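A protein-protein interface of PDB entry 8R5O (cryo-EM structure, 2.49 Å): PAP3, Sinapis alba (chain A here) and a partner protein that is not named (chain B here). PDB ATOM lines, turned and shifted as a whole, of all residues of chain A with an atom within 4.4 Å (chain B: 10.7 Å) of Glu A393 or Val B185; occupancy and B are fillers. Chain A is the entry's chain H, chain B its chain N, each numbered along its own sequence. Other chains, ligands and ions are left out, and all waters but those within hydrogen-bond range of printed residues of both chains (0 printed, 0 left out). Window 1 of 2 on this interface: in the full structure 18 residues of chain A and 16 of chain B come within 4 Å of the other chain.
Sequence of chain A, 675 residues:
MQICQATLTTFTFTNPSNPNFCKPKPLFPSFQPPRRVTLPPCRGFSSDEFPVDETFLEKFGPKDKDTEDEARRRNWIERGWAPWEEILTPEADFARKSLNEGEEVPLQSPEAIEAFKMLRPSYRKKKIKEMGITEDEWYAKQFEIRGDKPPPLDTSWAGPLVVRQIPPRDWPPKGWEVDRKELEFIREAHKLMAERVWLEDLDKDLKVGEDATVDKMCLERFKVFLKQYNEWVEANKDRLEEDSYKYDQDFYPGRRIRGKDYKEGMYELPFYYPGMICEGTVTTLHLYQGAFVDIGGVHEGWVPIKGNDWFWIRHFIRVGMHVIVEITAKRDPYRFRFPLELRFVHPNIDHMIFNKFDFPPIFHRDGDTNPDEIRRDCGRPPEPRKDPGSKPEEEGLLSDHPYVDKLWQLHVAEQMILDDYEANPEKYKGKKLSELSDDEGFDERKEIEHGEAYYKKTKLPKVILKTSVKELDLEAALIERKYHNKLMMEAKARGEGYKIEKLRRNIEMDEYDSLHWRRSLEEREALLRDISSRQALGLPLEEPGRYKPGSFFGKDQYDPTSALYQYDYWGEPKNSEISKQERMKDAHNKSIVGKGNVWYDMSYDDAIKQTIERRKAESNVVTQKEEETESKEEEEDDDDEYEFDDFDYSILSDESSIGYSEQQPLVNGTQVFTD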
ATOM      1  N   LYS A 391       6.185  -0.755 -16.202  1.00  0.00           N
ATOM      2  CA  LYS A 391       5.618   0.554 -16.503  1.00  0.00           C
ATOM      3  C   LYS A 391       6.579   1.654 -16.064  1.00  0.00           C
ATOM      4  O   LYS A 391       7.024   1.655 -14.912  1.00  0.00           O
ATOM      5  CB  LYS A 391       4.268   0.722 -15.815  1.00  0.00           C
ATOM      6  CG  LYS A 391       3.211  -0.251 -16.311  1.00  0.00           C
ATOM      7  CD  LYS A 391       1.909  -0.106 -15.543  1.00  0.00           C
ATOM      8  CE  LYS A 391       0.854  -1.068 -16.064  1.00  0.00           C
ATOM      9  NZ  LYS A 391      -0.426  -0.957 -15.311  1.00  0.00           N
ATOM     10  N   PRO A 392       6.927   2.591 -16.948  1.00  0.00           N
ATOM     11  CA  PRO A 392       7.894   3.637 -16.569  1.00  0.00           C
ATOM     12  C   PRO A 392       7.441   4.509 -15.411  1.00  0.00           C
ATOM     13  O   PRO A 392       8.290   5.021 -14.672  1.00  0.00           O
ATOM     14  CB  PRO A 392       8.052   4.450 -17.862  1.00  0.00           C
ATOM     15  CG  PRO A 392       6.817   4.164 -18.650  1.00  0.00           C
ATOM     16  CD  PRO A 392       6.453   2.748 -18.332  1.00  0.00           C
ATOM     17  N   GLU A 393       6.134   4.703 -15.225  1.00  0.00           N
ATOM     18  CA  GLU A 393       5.668   5.559 -14.141  1.00  0.00           C
ATOM     19  C   GLU A 393       5.769   4.894 -12.775  1.00  0.00           C
ATOM     20  O   GLU A 393       5.551   5.568 -11.763  1.00  0.00           O
ATOM     21  CB  GLU A 393       4.225   6.002 -14.391  1.00  0.00           C
ATOM     22  CG  GLU A 393       3.173   4.940 -14.113  1.00  0.00           C
ATOM     23  CD  GLU A 393       2.964   3.992 -15.277  1.00  0.00           C
ATOM     24  OE1 GLU A 393       3.665   4.135 -16.300  1.00  0.00           O
ATOM     25  OE2 GLU A 393       2.092   3.106 -15.169  1.00  0.00           O
ATOM     26  N   GLU A 394       6.089   3.603 -12.715  1.00  0.00           N
ATOM     27  CA  GLU A 394       6.199   2.882 -11.453  1.00  0.00           C
ATOM     28  C   GLU A 394       7.643   2.614 -11.050  1.00  0.00           C
ATOM     29  O   GLU A 394       7.879   1.901 -10.070  1.00  0.00           O
ATOM     30  CB  GLU A 394       5.429   1.563 -11.529  1.00  0.00           C
ATOM     31  CG  GLU A 394       3.963   1.722 -11.875  1.00  0.00           C
ATOM     32  CD  GLU A 394       3.195   0.425 -11.738  1.00  0.00           C
ATOM     33  OE1 GLU A 394       3.711  -0.504 -11.081  1.00  0.00           O
ATOM     34  OE2 GLU A 394       2.076   0.333 -12.287  1.00  0.00           O
ATOM     35  N   GLU A 395       8.611   3.164 -11.772  1.00  0.00           N
ATOM     36  CA  GLU A 395      10.016   2.953 -11.464  1.00  0.00           C
ATOM     37  C   GLU A 395      10.510   4.000 -10.473  1.00  0.00           C
ATOM     38  O   GLU A 395       9.990   5.117 -10.408  1.00  0.00           O
ATOM     39  CB  GLU A 395      10.859   2.997 -12.739  1.00  0.00           C
ATOM     40  CG  GLU A 395      10.495   1.919 -13.744  1.00  0.00           C
ATOM     41  CD  GLU A 395      11.175   2.114 -15.084  1.00  0.00           C
ATOM     42  OE1 GLU A 395      11.812   3.169 -15.283  1.00  0.00           O
ATOM     43  OE2 GLU A 395      11.069   1.211 -15.940  1.00  0.00           O
ATOM     44  N   ARG A 524       8.538  12.871 -13.536  1.00  0.00           N
ATOM     45  CA  ARG A 524       7.549  11.875 -13.135  1.00  0.00           C
ATOM     46  C   ARG A 524       6.187  12.510 -12.893  1.00  0.00           C
ATOM     47  O   ARG A 524       5.155  11.945 -13.271  1.00  0.00           O
ATOM     48  CB  ARG A 524       8.026  11.137 -11.884  1.00  0.00           C
ATOM     49  CG  ARG A 524       7.091  10.030 -11.425  1.00  0.00           C
ATOM     50  CD  ARG A 524       6.904   8.982 -12.506  1.00  0.00           C
ATOM     51  NE  ARG A 524       8.179   8.450 -12.969  1.00  0.00           N
ATOM     52  CZ  ARG A 524       8.823   7.442 -12.397  1.00  0.00           C
ATOM     53  NH1 ARG A 524       8.331   6.820 -11.338  1.00  0.00           N
ATOM     54  NH2 ARG A 524       9.991   7.051 -12.898  1.00  0.00           N
ATOM     55  N   LEU A 527       4.766  13.194 -16.128  1.00  0.00           N
ATOM     56  CA  LEU A 527       4.399  11.931 -16.762  1.00  0.00           C
ATOM     57  C   LEU A 527       3.055  11.426 -16.257  1.00  0.00           C
ATOM     58  O   LEU A 527       2.249  10.903 -17.034  1.00  0.00           O
ATOM     59  CB  LEU A 527       5.489  10.887 -16.521  1.00  0.00           C
ATOM     60  CG  LEU A 527       5.221   9.482 -17.064  1.00  0.00           C
ATOM     61  CD1 LEU A 527       5.021   9.515 -18.571  1.00  0.00           C
ATOM     62  CD2 LEU A 527       6.349   8.537 -16.690  1.00  0.00           C
ATOM     63  N   LEU A 528       2.796  11.570 -14.955  1.00  0.00           N
ATOM     64  CA  LEU A 528       1.536  11.094 -14.394  1.00  0.00           C
ATOM     65  C   LEU A 528       0.347  11.851 -14.971  1.00  0.00           C
ATOM     66  O   LEU A 528      -0.687  11.248 -15.280  1.00  0.00           O
ATOM     67  CB  LEU A 528       1.566  11.213 -12.870  1.00  0.00           C
ATOM     68  CG  LEU A 528       2.578  10.311 -12.160  1.00  0.00           C
ATOM     69  CD1 LEU A 528       2.681  10.676 -10.690  1.00  0.00           C
ATOM     70  CD2 LEU A 528       2.204   8.847 -12.324  1.00  0.00           C
ATOM     71  N   ILE A 531      -0.069  10.739 -18.635  1.00  0.00           N
ATOM     72  CA  ILE A 531      -0.718   9.437 -18.773  1.00  0.00           C
ATOM     73  C   ILE A 531      -2.234   9.588 -18.718  1.00  0.00           C
ATOM     74  O   ILE A 531      -2.962   9.007 -19.531  1.00  0.00           O
ATOM     75  CB  ILE A 531      -0.203   8.465 -17.695  1.00  0.00           C
ATOM     76  CG1 ILE A 531       1.227   8.033 -18.012  1.00  0.00           C
ATOM     77  CG2 ILE A 531      -1.112   7.253 -17.578  1.00  0.00           C
ATOM     78  CD1 ILE A 531       1.837   7.139 -16.963  1.00  0.00           C
ATOM     79  N   TYR B 106     -10.344   4.981 -11.221  1.00  0.00           N
ATOM     80  CA  TYR B 106      -9.264   5.441 -12.088  1.00  0.00           C
ATOM     81  C   TYR B 106      -8.273   4.318 -12.367  1.00  0.00           C
ATOM     82  O   TYR B 106      -7.785   4.183 -13.495  1.00  0.00           O
ATOM     83  CB  TYR B 106      -8.561   6.647 -11.467  1.00  0.00           C
ATOM     84  CG  TYR B 106      -7.393   7.160 -12.280  1.00  0.00           C
ATOM     85  CD1 TYR B 106      -7.587   7.725 -13.534  1.00  0.00           C
ATOM     86  CD2 TYR B 106      -6.097   7.085 -11.790  1.00  0.00           C
ATOM     87  CE1 TYR B 106      -6.521   8.195 -14.278  1.00  0.00           C
ATOM     88  CE2 TYR B 106      -5.028   7.554 -12.524  1.00  0.00           C
ATOM     89  CZ  TYR B 106      -5.244   8.105 -13.767  1.00  0.00           C
ATOM     90  OH  TYR B 106      -4.175   8.569 -14.495  1.00  0.00           O
ATOM     91  N   ASN B 107      -7.965   3.510 -11.351  1.00  0.00           N
ATOM     92  CA  ASN B 107      -7.169   2.293 -11.514  1.00  0.00           C
ATOM     93  C   ASN B 107      -5.798   2.591 -12.119  1.00  0.00           C
ATOM     94  O   ASN B 107      -5.337   1.903 -13.033  1.00  0.00           O
ATOM     95  CB  ASN B 107      -7.929   1.260 -12.351  1.00  0.00           C
ATOM     96  CG  ASN B 107      -7.323  -0.124 -12.269  1.00  0.00           C
ATOM     97  OD1 ASN B 107      -6.640  -0.460 -11.302  1.00  0.00           O
ATOM     98  ND2 ASN B 107      -7.571  -0.937 -13.287  1.00  0.00           N
ATOM     99  N   ARG B 108      -5.146   3.640 -11.611  1.00  0.00           N
ATOM    100  CA  ARG B 108      -3.783   4.006 -11.999  1.00  0.00           C
ATOM    101  C   ARG B 108      -3.651   4.250 -13.500  1.00  0.00           C
ATOM    102  O   ARG B 108      -2.605   3.978 -14.092  1.00  0.00           O
ATOM    103  CB  ARG B 108      -2.776   2.946 -11.543  1.00  0.00           C
ATOM    104  CG  ARG B 108      -2.812   2.662 -10.052  1.00  0.00           C
ATOM    105  CD  ARG B 108      -1.826   1.570  -9.675  1.00  0.00           C
ATOM    106  NE  ARG B 108      -0.455   1.942 -10.001  1.00  0.00           N
ATOM    107  CZ  ARG B 108       0.349   2.623  -9.195  1.00  0.00           C
ATOM    108  NH1 ARG B 108      -0.052   3.024  -7.999  1.00  0.00           N
ATOM    109  NH2 ARG B 108       1.581   2.912  -9.599  1.00  0.00           N
ATOM    110  N   GLY B 109      -4.707   4.765 -14.133  1.00  0.00           N
ATOM    111  CA  GLY B 109      -4.697   5.123 -15.536  1.00  0.00           C
ATOM    112  C   GLY B 109      -5.499   4.186 -16.419  1.00  0.00           C
ATOM    113  O   GLY B 109      -5.947   4.598 -17.495  1.00  0.00           O
ATOM    114  N   ASN B 110      -5.690   2.938 -15.991  1.00  0.00           N
ATOM    115  CA  ASN B 110      -6.511   1.984 -16.737  1.00  0.00           C
ATOM    116  C   ASN B 110      -7.939   2.091 -16.213  1.00  0.00           C
ATOM    117  O   ASN B 110      -8.426   1.253 -15.453  1.00  0.00           O
ATOM    118  CB  ASN B 110      -5.951   0.574 -16.605  1.00  0.00           C
ATOM    119  CG  ASN B 110      -4.488   0.494 -16.987  1.00  0.00           C
ATOM    120  OD1 ASN B 110      -4.146   0.380 -18.164  1.00  0.00           O
ATOM    121  ND2 ASN B 110      -3.612   0.557 -15.990  1.00  0.00           N
ATOM    122  N   ASN B 181       1.268  16.664  -3.238  1.00  0.00           N
ATOM    123  CA  ASN B 181       1.120  15.258  -3.570  1.00  0.00           C
ATOM    124  C   ASN B 181       2.264  14.426  -3.000  1.00  0.00           C
ATOM    125  O   ASN B 181       3.368  14.916  -2.748  1.00  0.00           O
ATOM    126  CB  ASN B 181       1.059  15.073  -5.085  1.00  0.00           C
ATOM    127  CG  ASN B 181       2.279  15.641  -5.788  1.00  0.00           C
ATOM    128  OD1 ASN B 181       2.765  16.715  -5.435  1.00  0.00           O
ATOM    129  ND2 ASN B 181       2.780  14.918  -6.780  1.00  0.00           N
ATOM    130  N   ARG B 182       1.979  13.144  -2.800  1.00  0.00           N
ATOM    131  CA  ARG B 182       2.986  12.147  -2.474  1.00  0.00           C
ATOM    132  C   ARG B 182       2.929  11.036  -3.511  1.00  0.00           C
ATOM    133  O   ARG B 182       1.847  10.654  -3.966  1.00  0.00           O
ATOM    134  CB  ARG B 182       2.781  11.574  -1.067  1.00  0.00           C
ATOM    135  CG  ARG B 182       1.425  10.936  -0.839  1.00  0.00           C
ATOM    136  CD  ARG B 182       1.400  10.149   0.459  1.00  0.00           C
ATOM    137  NE  ARG B 182       1.798  10.966   1.600  1.00  0.00           N
ATOM    138  CZ  ARG B 182       1.818  10.541   2.855  1.00  0.00           C
ATOM    139  NH1 ARG B 182       1.461   9.309   3.173  1.00  0.00           N
ATOM    140  NH2 ARG B 182       2.208  11.375   3.814  1.00  0.00           N
ATOM    141  N   LEU B 183       4.095  10.532  -3.892  1.00  0.00           N
ATOM    142  CA  LEU B 183       4.204   9.508  -4.919  1.00  0.00           C
ATOM    143  C   LEU B 183       4.348   8.131  -4.284  1.00  0.00           C
ATOM    144  O   LEU B 183       4.966   7.973  -3.228  1.00  0.00           O
ATOM    145  CB  LEU B 183       5.393   9.786  -5.841  1.00  0.00           C
ATOM    146  CG  LEU B 183       5.155  10.641  -7.088  1.00  0.00           C
ATOM    147  CD1 LEU B 183       4.427  11.936  -6.763  1.00  0.00           C
ATOM    148  CD2 LEU B 183       6.477  10.937  -7.767  1.00  0.00           C
ATOM    149  N   ASP B 184       3.775   7.127  -4.951  1.00  0.00           N
ATOM    150  CA  ASP B 184       3.817   5.747  -4.485  1.00  0.00           C
ATOM    151  C   ASP B 184       4.996   4.970  -5.062  1.00  0.00           C
ATOM    152  O   ASP B 184       4.916   3.744  -5.213  1.00  0.00           O
ATOM    153  CB  ASP B 184       2.498   5.046  -4.811  1.00  0.00           C
ATOM    154  CG  ASP B 184       2.251   3.826  -3.941  1.00  0.00           C
ATOM    155  OD1 ASP B 184       2.041   3.995  -2.722  1.00  0.00           O
ATOM    156  OD2 ASP B 184       2.263   2.698  -4.478  1.00  0.00           O
ATOM    157  N   VAL B 185       6.087   5.652  -5.394  1.00  0.00           N
ATOM    158  CA  VAL B 185       7.277   5.008  -5.928  1.00  0.00           C
ATOM    159  C   VAL B 185       8.405   5.131  -4.907  1.00  0.00           C
ATOM    160  O   VAL B 185       8.297   5.839  -3.907  1.00  0.00           O
ATOM    161  CB  VAL B 185       7.693   5.597  -7.291  1.00  0.00           C
ATOM    162  CG1 VAL B 185       6.548   5.499  -8.283  1.00  0.00           C
ATOM    163  CG2 VAL B 185       8.150   7.036  -7.132  1.00  0.00           C
ATOM    164  N   ALA B 186       9.498   4.427  -5.175  1.00  0.00           N
ATOM    165  CA  ALA B 186      10.638   4.418  -4.271  1.00  0.00           C
ATOM    166  C   ALA B 186      11.494   5.662  -4.463  1.00  0.00           C
ATOM    167  O   ALA B 186      11.558   6.237  -5.554  1.00  0.00           O
ATOM    168  CB  ALA B 186      11.485   3.166  -4.492  1.00  0.00           C
ATOM    169  N   ASN B 187      12.160   6.072  -3.381  1.00  0.00           N
ATOM    170  CA  ASN B 187      13.046   7.237  -3.383  1.00  0.00           C
ATOM    171  C   ASN B 187      12.311   8.492  -3.849  1.00  0.00           C
ATOM    172  O   ASN B 187      12.825   9.281  -4.643  1.00  0.00           O
ATOM    173  CB  ASN B 187      14.291   6.978  -4.238  1.00  0.00           C
ATOM    174  CG  ASN B 187      15.390   7.991  -3.992  1.00  0.00           C
ATOM    175  OD1 ASN B 187      15.475   8.586  -2.919  1.00  0.00           O
ATOM    176  ND2 ASN B 187      16.240   8.195  -4.991  1.00  0.00           N
ATOM    177  N   ALA B 188      11.089   8.679  -3.349  1.00  0.00           N
ATOM    178  CA  ALA B 188      10.248   9.805  -3.737  1.00  0.00           C
ATOM    179  C   ALA B 188       9.974  10.766  -2.588  1.00  0.00           C
ATOM    180  O   ALA B 188       9.073  11.605  -2.700  1.00  0.00           O
ATOM    181  CB  ALA B 188       8.926   9.298  -4.317  1.00  0.00           C
ATOM    182  N   VAL B 189      10.719  10.671  -1.492  1.00  0.00           N
ATOM    183  CA  VAL B 189      10.527  11.524  -0.324  1.00  0.00           C
ATOM    184  C   VAL B 189      11.704  12.482  -0.228  1.00  0.00           C
ATOM    185  O   VAL B 189      12.864  12.058  -0.275  1.00  0.00           O
ATOM    186  CB  VAL B 189      10.384  10.697   0.964  1.00  0.00           C
ATOM    187  CG1 VAL B 189      10.149  11.610   2.157  1.00  0.00           C
ATOM    188  CG2 VAL B 189       9.258   9.689   0.827  1.00  0.00           C
ATOM    189  N   ASN B 190      11.406  13.771  -0.099  1.00  0.00           N
ATOM    190  CA  ASN B 190      12.447  14.778   0.046  1.00  0.00           C
ATOM    191  C   ASN B 190      12.957  14.783   1.483  1.00  0.00           C
ATOM    192  O   ASN B 190      12.170  15.024   2.405  1.00  0.00           O
ATOM    193  CB  ASN B 190      11.911  16.154  -0.327  1.00  0.00           C
ATOM    194  CG  ASN B 190      13.011  17.181  -0.505  1.00  0.00           C
ATOM    195  OD1 ASN B 190      14.184  16.834  -0.624  1.00  0.00           O
ATOM    196  ND2 ASN B 190      12.633  18.452  -0.532  1.00  0.00           N
ATOM    197  N   VAL B 213      -6.816  12.328  -9.058  1.00  0.00           N
ATOM    198  CA  VAL B 213      -6.117  11.110  -9.454  1.00  0.00           C
ATOM    199  C   VAL B 213      -4.603  11.232  -9.353  1.00  0.00           C
ATOM    200  O   VAL B 213      -3.911  10.210  -9.410  1.00  0.00           O
ATOM    201  CB  VAL B 213      -6.519  10.689 -10.882  1.00  0.00           C
ATOM    202  CG1 VAL B 213      -8.014  10.418 -10.952  1.00  0.00           C
ATOM    203  CG2 VAL B 213      -6.119  11.747 -11.891  1.00  0.00           C
ATOM    204  N   TRP B 214      -4.065  12.442  -9.202  1.00  0.00           N
ATOM    205  CA  TRP B 214      -2.646  12.629  -8.931  1.00  0.00           C
ATOM    206  C   TRP B 214      -2.382  13.058  -7.495  1.00  0.00           C
ATOM    207  O   TRP B 214      -1.277  13.520  -7.193  1.00  0.00           O
ATOM    208  CB  TRP B 214      -2.026  13.656  -9.881  1.00  0.00           C
ATOM    209  CG  TRP B 214      -2.653  13.742 -11.229  1.00  0.00           C
ATOM    210  CD1 TRP B 214      -2.834  12.728 -12.119  1.00  0.00           C
ATOM    211  CD2 TRP B 214      -3.152  14.925 -11.857  1.00  0.00           C
ATOM    212  NE1 TRP B 214      -3.434  13.203 -13.259  1.00  0.00           N
ATOM    213  CE2 TRP B 214      -3.638  14.551 -13.123  1.00  0.00           C
ATOM    214  CE3 TRP B 214      -3.240  16.263 -11.468  1.00  0.00           C
ATOM    215  CZ2 TRP B 214      -4.204  15.467 -14.001  1.00  0.00           C
ATOM    216  CZ3 TRP B 214      -3.803  17.170 -12.341  1.00  0.00           C
ATOM    217  CH2 TRP B 214      -4.278  16.768 -13.593  1.00  0.00           C
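Of the 9 printed residues of chain A, 6 touch a printed residue of chain B.
Printed residues of chain A that touch a printed residue of chain B: Lys A391, Glu A393, Glu A394, Glu A395, Arg A524 and Leu A528.
Along chain A the printed residues that touch a printed residue of chain B span positions 391 to 528.
Of the 17 printed residues of chain B, 5 touch a printed residue of chain A.
Printed residues of chain B that touch a printed residue of chain A: Arg B108, Asn B110, Leu B183, Val B185 and Trp B214.
Hydrophobic or aromatic side chains of chain B within 4 Å of the printed part of chain A: Leu B183, Val B185 and Trp B214.
Along chain B the printed residues that touch a printed residue of chain A span positions 108 to 214.
Among the printed residues, Asp or Glu carboxylates within 4 Å of a Lys or Arg side-chain nitrogen of the other chain: Glu A394 with Arg B108.
The guanidinium group (NH2) of Arg B108 is in salt-bridge range of the side-chain carboxylate (OE2) of Glu A394 (3.8 Å).
Lys A391 touches Asn B110 (NZ to ND2, 3.6 Å).
Glu A393 touches Val B185 (O to CG1, 3.6 Å).
Glu A395 touches Val B185 (O to CB, 3.9 Å).
Leu B183 touches Arg A524 (CD2 to CG, 3.8 Å).
Arg A524 touches Val B185.
NE1 of Trp B214 touches O of Leu A528, 3.9 Å away.
The backbone carbonyl oxygen (O) of Asn B110 lies close to the side-chain amide nitrogen (ND2) of Asn B107 (3.2 Å).
The guanidinium group (NH2) of Arg A524 sits at hydrogen-bond distance from the backbone carbonyl oxygen (O) of Pro A392.
The guanidinium group (NH1) of Arg A524 lies within hydrogen-bond range of the backbone carbonyl oxygen (O) of Glu A393, at 3.1 Å.
O of Glu A395 sits at hydrogen-bond distance from NH1 of Arg A524 (2.6 Å).
Lys A391 touches just one residue of chain B: Asn B110.
No residue of chain B comes within 4 Å of Pro A392.
Glu A393 touches one residue of chain B.
Glu A394 touches one residue of chain B.
Glu A395 touches just one residue of chain B: Val B185.
Printed residues of chain B within 4 Å of Arg A524: Leu B183 and Val B185.
Printed residues of chain B within 4 Å of Leu A528: Trp B214 (3.9 Å).
Printed residues of chain A within 4 Å of Leu B183: Arg A524 (3.8 Å).
Of chain A, only Glu A393, Glu A395 and Arg A524 come within 4 Å of Val B185.
The nearest residue of chain A that does not touch Val B185 is Glu A394 (4.1 Å).
The nearest printed residue of chain A that does not touch Leu B183 is Leu A528 (4.4 Å).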
